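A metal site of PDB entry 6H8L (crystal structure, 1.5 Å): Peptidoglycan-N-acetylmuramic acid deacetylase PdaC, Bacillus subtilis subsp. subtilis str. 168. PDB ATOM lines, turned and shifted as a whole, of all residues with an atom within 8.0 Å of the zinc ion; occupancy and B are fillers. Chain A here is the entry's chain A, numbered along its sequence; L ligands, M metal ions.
The backbone NH (N) of Asp 18 lies within hydrogen-bond range of the backbone carbonyl oxygen (O) of Phe 42, 3.2 Å away.
The side-chain hydroxyl of Tyr 109 sits at hydrogen-bond distance from a ring nitrogen (ND1) of His 72, 3.2 Å away.
N of His 72 is in hydrogen-bond range of OG of Ser 69 (2.9 Å).
A ring nitrogen (ND1) of His 68 is in hydrogen-bond range of the backbone carbonyl oxygen of Arg 106 (2.7 Å).
The backbone carbonyl oxygen (O) of Val 43 sits at hydrogen-bond distance from the backbone NH (N) of His 68 (3.0 Å).
Three residues have an atom within 4 Å of the zinc ion: Asp 18, His 68 and His 72.
The nearest printed residue that does not touch the zinc ion is Asp 17 (4.4 Å).
The zinc ion is bound by an oxygen (O2) of the ligand (1.9 Å), the side-chain carboxylate (OD1) of Asp 18 (2.0 Å), a ring nitrogen (NE2) of His 72 (2.0 Å) and a ring nitrogen (NE2) of His 68 (2.1 Å).
The zinc ion has four donor atoms within binding distance.
Slightly farther from the zinc ion lies an oxygen (O1) of the ligand (2.6 Å).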
ATOM      1  N   PHE A  16      29.466   7.975 -28.852  1.00  0.00           N
ATOM      2  CA  PHE A  16      28.905   8.002 -27.518  1.00  0.00           C
ATOM      3  C   PHE A  16      28.594   9.443 -27.141  1.00  0.00           C
ATOM      4  O   PHE A  16      29.503  10.281 -27.101  1.00  0.00           O
ATOM      5  CB  PHE A  16      29.871   7.387 -26.508  1.00  0.00           C
ATOM      6  CG  PHE A  16      30.130   5.927 -26.749  1.00  0.00           C
ATOM      7  CD1 PHE A  16      29.251   4.981 -26.270  1.00  0.00           C
ATOM      8  CD2 PHE A  16      31.244   5.517 -27.444  1.00  0.00           C
ATOM      9  CE1 PHE A  16      29.470   3.649 -26.490  1.00  0.00           C
ATOM     10  CE2 PHE A  16      31.474   4.177 -27.665  1.00  0.00           C
ATOM     11  CZ  PHE A  16      30.576   3.241 -27.190  1.00  0.00           C
ATOM     12  N   ASP A  17      27.330   9.723 -26.829  1.00  0.00           N
ATOM     13  CA  ASP A  17      26.857  11.073 -26.557  1.00  0.00           C
ATOM     14  C   ASP A  17      26.410  11.219 -25.109  1.00  0.00           C
ATOM     15  O   ASP A  17      25.880  10.277 -24.503  1.00  0.00           O
ATOM     16  CB  ASP A  17      25.699  11.455 -27.485  1.00  0.00           C
ATOM     17  CG  ASP A  17      26.117  11.600 -28.931  1.00  0.00           C
ATOM     18  OD1 ASP A  17      27.277  11.315 -29.246  1.00  0.00           O
ATOM     19  OD2 ASP A  17      25.257  11.993 -29.763  1.00  0.00           O
ATOM     20  N   ASP A  18      26.619  12.422 -24.576  1.00  0.00           N
ATOM     21  CA  ASP A  18      26.074  12.983 -23.329  1.00  0.00           C
ATOM     22  C   ASP A  18      26.988  12.871 -22.112  1.00  0.00           C
ATOM     23  O   ASP A  18      26.623  13.352 -21.039  1.00  0.00           O
ATOM     24  CB  ASP A  18      24.725  12.353 -22.951  1.00  0.00           C
ATOM     25  CG  ASP A  18      23.624  12.697 -23.923  1.00  0.00           C
ATOM     26  OD1 ASP A  18      23.852  13.548 -24.810  1.00  0.00           O
ATOM     27  OD2 ASP A  18      22.524  12.104 -23.805  1.00  0.00           O
ATOM     28  N   GLY A  19      28.174  12.289 -22.274  1.00  0.00           N
ATOM     29  CA  GLY A  19      29.126  12.192 -21.192  1.00  0.00           C
ATOM     30  C   GLY A  19      30.044  13.401 -21.152  1.00  0.00           C
ATOM     31  O   GLY A  19      29.780  14.403 -21.821  1.00  0.00           O
ATOM     32  N   PHE A  42      30.986  12.496 -28.034  1.00  0.00           N
ATOM     33  CA  PHE A  42      30.430  13.835 -28.167  1.00  0.00           C
ATOM     34  C   PHE A  42      29.993  14.280 -26.777  1.00  0.00           C
ATOM     35  O   PHE A  42      28.970  13.815 -26.252  1.00  0.00           O
ATOM     36  CB  PHE A  42      29.283  13.842 -29.166  1.00  0.00           C
ATOM     37  CG  PHE A  42      29.749  13.650 -30.581  1.00  0.00           C
ATOM     38  CD1 PHE A  42      30.126  14.744 -31.362  1.00  0.00           C
ATOM     39  CD2 PHE A  42      29.861  12.383 -31.130  1.00  0.00           C
ATOM     40  CE1 PHE A  42      30.579  14.570 -32.654  1.00  0.00           C
ATOM     41  CE2 PHE A  42      30.308  12.202 -32.433  1.00  0.00           C
ATOM     42  CZ  PHE A  42      30.670  13.299 -33.190  1.00  0.00           C
ATOM     43  N   VAL A  43      30.782  15.170 -26.185  1.00  0.00           N
ATOM     44  CA  VAL A  43      30.695  15.481 -24.761  1.00  0.00           C
ATOM     45  C   VAL A  43      29.930  16.777 -24.527  1.00  0.00           C
ATOM     46  O   VAL A  43      29.958  17.704 -25.343  1.00  0.00           O
ATOM     47  CB  VAL A  43      32.111  15.579 -24.150  1.00  0.00           C
ATOM     48  CG1 VAL A  43      32.832  14.263 -24.259  1.00  0.00           C
ATOM     49  CG2 VAL A  43      32.923  16.685 -24.826  1.00  0.00           C
ATOM     50  N   LEU A  44      29.279  16.831 -23.366  1.00  0.00           N
ATOM     51  CA  LEU A  44      28.675  18.068 -22.872  1.00  0.00           C
ATOM     52  C   LEU A  44      29.716  18.899 -22.147  1.00  0.00           C
ATOM     53  O   LEU A  44      30.447  18.390 -21.288  1.00  0.00           O
ATOM     54  CB  LEU A  44      27.523  17.734 -21.916  1.00  0.00           C
ATOM     55  CG  LEU A  44      26.227  17.317 -22.588  1.00  0.00           C
ATOM     56  CD1 LEU A  44      25.308  16.646 -21.573  1.00  0.00           C
ATOM     57  CD2 LEU A  44      25.535  18.508 -23.227  1.00  0.00           C
ATOM     58  N   HIS A  68      29.069  18.502 -28.041  1.00  0.00           N
ATOM     59  CA  HIS A  68      27.644  18.182 -27.923  1.00  0.00           C
ATOM     60  C   HIS A  68      26.880  19.267 -27.169  1.00  0.00           C
ATOM     61  O   HIS A  68      25.847  18.998 -26.562  1.00  0.00           O
ATOM     62  CB  HIS A  68      27.469  16.819 -27.267  1.00  0.00           C
ATOM     63  CG  HIS A  68      26.113  16.193 -27.432  1.00  0.00           C
ATOM     64  ND1 HIS A  68      25.425  16.177 -28.624  1.00  0.00           N
ATOM     65  CD2 HIS A  68      25.354  15.518 -26.544  1.00  0.00           C
ATOM     66  CE1 HIS A  68      24.285  15.520 -28.457  1.00  0.00           C
ATOM     67  NE2 HIS A  68      24.211  15.119 -27.209  1.00  0.00           N
ATOM     68  N   SER A  69      27.387  20.505 -27.206  1.00  0.00           N
ATOM     69  CA  SER A  69      26.830  21.671 -26.517  1.00  0.00           C
ATOM     70  C   SER A  69      27.203  21.703 -25.044  1.00  0.00           C
ATOM     71  O   SER A  69      27.828  20.765 -24.521  1.00  0.00           O
ATOM     72  CB  SER A  69      25.307  21.730 -26.687  1.00  0.00           C
ATOM     73  OG  SER A  69      24.635  21.056 -25.631  1.00  0.00           O
ATOM     74  N   HIS A  72      22.901  20.989 -23.304  1.00  0.00           N
ATOM     75  CA  HIS A  72      21.996  20.116 -24.050  1.00  0.00           C
ATOM     76  C   HIS A  72      20.640  20.734 -24.409  1.00  0.00           C
ATOM     77  O   HIS A  72      19.640  20.010 -24.465  1.00  0.00           O
ATOM     78  CB  HIS A  72      21.738  18.839 -23.238  1.00  0.00           C
ATOM     79  CG  HIS A  72      21.527  17.627 -24.094  1.00  0.00           C
ATOM     80  ND1 HIS A  72      20.307  17.291 -24.638  1.00  0.00           N
ATOM     81  CD2 HIS A  72      22.387  16.651 -24.479  1.00  0.00           C
ATOM     82  CE1 HIS A  72      20.424  16.179 -25.332  1.00  0.00           C
ATOM     83  NE2 HIS A  72      21.677  15.761 -25.255  1.00  0.00           N
ATOM     84  N   ARG A 106      27.887  17.497 -32.721  1.00  0.00           N
ATOM     85  CA  ARG A 106      26.607  16.816 -32.851  1.00  0.00           C
ATOM     86  C   ARG A 106      25.569  17.665 -32.114  1.00  0.00           C
ATOM     87  O   ARG A 106      25.563  17.698 -30.869  1.00  0.00           O
ATOM     88  CB  ARG A 106      26.677  15.393 -32.298  1.00  0.00           C
ATOM     89  CG  ARG A 106      25.505  14.564 -32.696  1.00  0.00           C
ATOM     90  CD  ARG A 106      25.773  13.114 -32.410  1.00  0.00           C
ATOM     91  NE  ARG A 106      26.431  12.365 -33.486  1.00  0.00           N
ATOM     92  CZ  ARG A 106      26.901  11.141 -33.301  1.00  0.00           C
ATOM     93  NH1 ARG A 106      26.812  10.592 -32.104  1.00  0.00           N
ATOM     94  NH2 ARG A 106      27.441  10.440 -34.288  1.00  0.00           N
ATOM     95  N   PRO A 107      24.709  18.396 -32.806  1.00  0.00           N
ATOM     96  CA  PRO A 107      23.722  19.222 -32.119  1.00  0.00           C
ATOM     97  C   PRO A 107      22.757  18.356 -31.327  1.00  0.00           C
ATOM     98  O   PRO A 107      22.323  17.311 -31.821  1.00  0.00           O
ATOM     99  CB  PRO A 107      23.003  19.941 -33.273  1.00  0.00           C
ATOM    100  CG  PRO A 107      23.968  19.902 -34.419  1.00  0.00           C
ATOM    101  CD  PRO A 107      24.706  18.606 -34.264  1.00  0.00           C
ATOM    102  N   PRO A 108      22.416  18.742 -30.088  1.00  0.00           N
ATOM    103  CA  PRO A 108      21.470  17.945 -29.309  1.00  0.00           C
ATOM    104  C   PRO A 108      20.191  17.659 -30.092  1.00  0.00           C
ATOM    105  O   PRO A 108      19.650  18.533 -30.765  1.00  0.00           O
ATOM    106  CB  PRO A 108      21.197  18.820 -28.079  1.00  0.00           C
ATOM    107  CG  PRO A 108      22.472  19.581 -27.903  1.00  0.00           C
ATOM    108  CD  PRO A 108      22.928  19.892 -29.310  1.00  0.00           C
ATOM    109  N   TYR A 109      19.736  16.414 -30.007  1.00  0.00           N
ATOM    110  CA  TYR A 109      18.543  15.909 -30.675  1.00  0.00           C
ATOM    111  C   TYR A 109      18.629  15.976 -32.196  1.00  0.00           C
ATOM    112  O   TYR A 109      17.634  15.740 -32.888  1.00  0.00           O
ATOM    113  CB  TYR A 109      17.288  16.647 -30.189  1.00  0.00           C
ATOM    114  CG  TYR A 109      17.227  16.804 -28.692  1.00  0.00           C
ATOM    115  CD1 TYR A 109      16.918  15.721 -27.864  1.00  0.00           C
ATOM    116  CD2 TYR A 109      17.501  18.026 -28.088  1.00  0.00           C
ATOM    117  CE1 TYR A 109      16.889  15.851 -26.502  1.00  0.00           C
ATOM    118  CE2 TYR A 109      17.470  18.163 -26.720  1.00  0.00           C
ATOM    119  CZ  TYR A 109      17.159  17.081 -25.926  1.00  0.00           C
ATOM    120  OH  TYR A 109      17.133  17.224 -24.564  1.00  0.00           O
ATOM    121  N   GLY A 110      19.816  16.251 -32.744  1.00  0.00           N
ATOM    122  CA  GLY A 110      19.985  16.413 -34.167  1.00  0.00           C
ATOM    123  C   GLY A 110      19.458  17.723 -34.718  1.00  0.00           C
ATOM    124  O   GLY A 110      19.507  17.920 -35.936  1.00  0.00           O
ATOM    125  N   TRP A 134      18.385   5.487 -24.892  1.00  0.00           N
ATOM    126  CA  TRP A 134      17.726   6.307 -23.873  1.00  0.00           C
ATOM    127  C   TRP A 134      16.260   5.909 -23.672  1.00  0.00           C
ATOM    128  O   TRP A 134      15.682   6.208 -22.625  1.00  0.00           O
ATOM    129  CB  TRP A 134      17.785   7.776 -24.279  1.00  0.00           C
ATOM    130  CG  TRP A 134      17.185   8.017 -25.627  1.00  0.00           C
ATOM    131  CD1 TRP A 134      17.823   8.029 -26.827  1.00  0.00           C
ATOM    132  CD2 TRP A 134      15.792   8.233 -25.909  1.00  0.00           C
ATOM    133  NE1 TRP A 134      16.932   8.254 -27.843  1.00  0.00           N
ATOM    134  CE2 TRP A 134      15.672   8.384 -27.306  1.00  0.00           C
ATOM    135  CE3 TRP A 134      14.647   8.326 -25.108  1.00  0.00           C
ATOM    136  CZ2 TRP A 134      14.443   8.629 -27.924  1.00  0.00           C
ATOM    137  CZ3 TRP A 134      13.434   8.569 -25.732  1.00  0.00           C
ATOM    138  CH2 TRP A 134      13.341   8.708 -27.120  1.00  0.00           C
ATOM    139  N   LEU A 157      24.954   5.237 -32.792  1.00  0.00           N
ATOM    140  CA  LEU A 157      24.673   6.220 -31.752  1.00  0.00           C
ATOM    141  C   LEU A 157      24.333   5.518 -30.435  1.00  0.00           C
ATOM    142  O   LEU A 157      23.284   4.889 -30.331  1.00  0.00           O
ATOM    143  CB  LEU A 157      23.504   7.116 -32.152  1.00  0.00           C
ATOM    144  CG  LEU A 157      22.962   8.055 -31.066  1.00  0.00           C
ATOM    145  CD1 LEU A 157      24.041   9.034 -30.632  1.00  0.00           C
ATOM    146  CD2 LEU A 157      21.722   8.782 -31.565  1.00  0.00           C
ATOM    147  N   ILE A 158      25.201   5.684 -29.439  1.00  0.00           N
ATOM    148  CA  ILE A 158      24.974   5.186 -28.083  1.00  0.00           C
ATOM    149  C   ILE A 158      25.186   6.370 -27.139  1.00  0.00           C
ATOM    150  O   ILE A 158      25.821   7.363 -27.480  1.00  0.00           O
ATOM    151  CB  ILE A 158      25.919   4.017 -27.733  1.00  0.00           C
ATOM    152  CG1 ILE A 158      25.725   2.873 -28.735  1.00  0.00           C
ATOM    153  CG2 ILE A 158      25.716   3.531 -26.297  1.00  0.00           C
ATOM    154  CD1 ILE A 158      26.729   1.750 -28.603  1.00  0.00           C
ATOM    155  N   HIS A 159      24.606   6.270 -25.938  1.00  0.00           N
ATOM    156  CA  HIS A 159      24.764   7.313 -24.921  1.00  0.00           C
ATOM    157  C   HIS A 159      25.479   6.731 -23.709  1.00  0.00           C
ATOM    158  O   HIS A 159      24.950   5.832 -23.057  1.00  0.00           O
ATOM    159  CB  HIS A 159      23.403   7.895 -24.534  1.00  0.00           C
ATOM    160  CG  HIS A 159      22.714   8.559 -25.672  1.00  0.00           C
ATOM    161  ND1 HIS A 159      21.974   7.859 -26.602  1.00  0.00           N
ATOM    162  CD2 HIS A 159      22.719   9.851 -26.092  1.00  0.00           C
ATOM    163  CE1 HIS A 159      21.521   8.696 -27.524  1.00  0.00           C
ATOM    164  NE2 HIS A 159      21.963   9.903 -27.233  1.00  0.00           N
ATOM    165  N   ILE A 161      25.888   7.393 -20.663  1.00  0.00           N
ATOM    166  CA  ILE A 161      25.426   7.870 -19.357  1.00  0.00           C
ATOM    167  C   ILE A 161      24.529   6.871 -18.652  1.00  0.00           C
ATOM    168  O   ILE A 161      24.076   7.151 -17.544  1.00  0.00           O
ATOM    169  CB  ILE A 161      24.697   9.221 -19.496  1.00  0.00           C
ATOM    170  CG1 ILE A 161      23.530   9.103 -20.494  1.00  0.00           C
ATOM    171  CG2 ILE A 161      25.686  10.279 -19.953  1.00  0.00           C
ATOM    172  CD1 ILE A 161      22.601  10.308 -20.499  1.00  0.00           C
HETATM  173  O1  LIG L   1      21.134  14.663 -28.288  1.00  0.00           O
HETATM  174  O2  LIG L   1      21.380  12.989 -26.874  1.00  0.00           O
HETATM  175  C1  LIG L   1      20.885  13.481 -27.927  1.00  0.00           C
HETATM  176  C2  LIG L   1      19.979  12.628 -28.800  1.00  0.00           C
HETATM  177  O3  LIG L   1      19.783  11.375 -28.177  1.00  0.00           O
HETATM  178  C3  LIG L   1      20.623  12.437 -30.175  1.00  0.00           C
HETATM  179  O4  LIG L   1      20.179  13.438 -31.051  1.00  0.00           O
HETATM  180  C4  LIG L   1      22.143  12.586 -30.085  1.00  0.00           C
HETATM  181  O5  LIG L   1      22.723  13.391 -30.863  1.00  0.00           O
HETATM  182  O6  LIG L   1      22.781  11.906 -29.233  1.00  0.00           O
HETATM  183 ZN    ZN M   1      22.647  14.270 -26.174  1.00  0.00          ZN
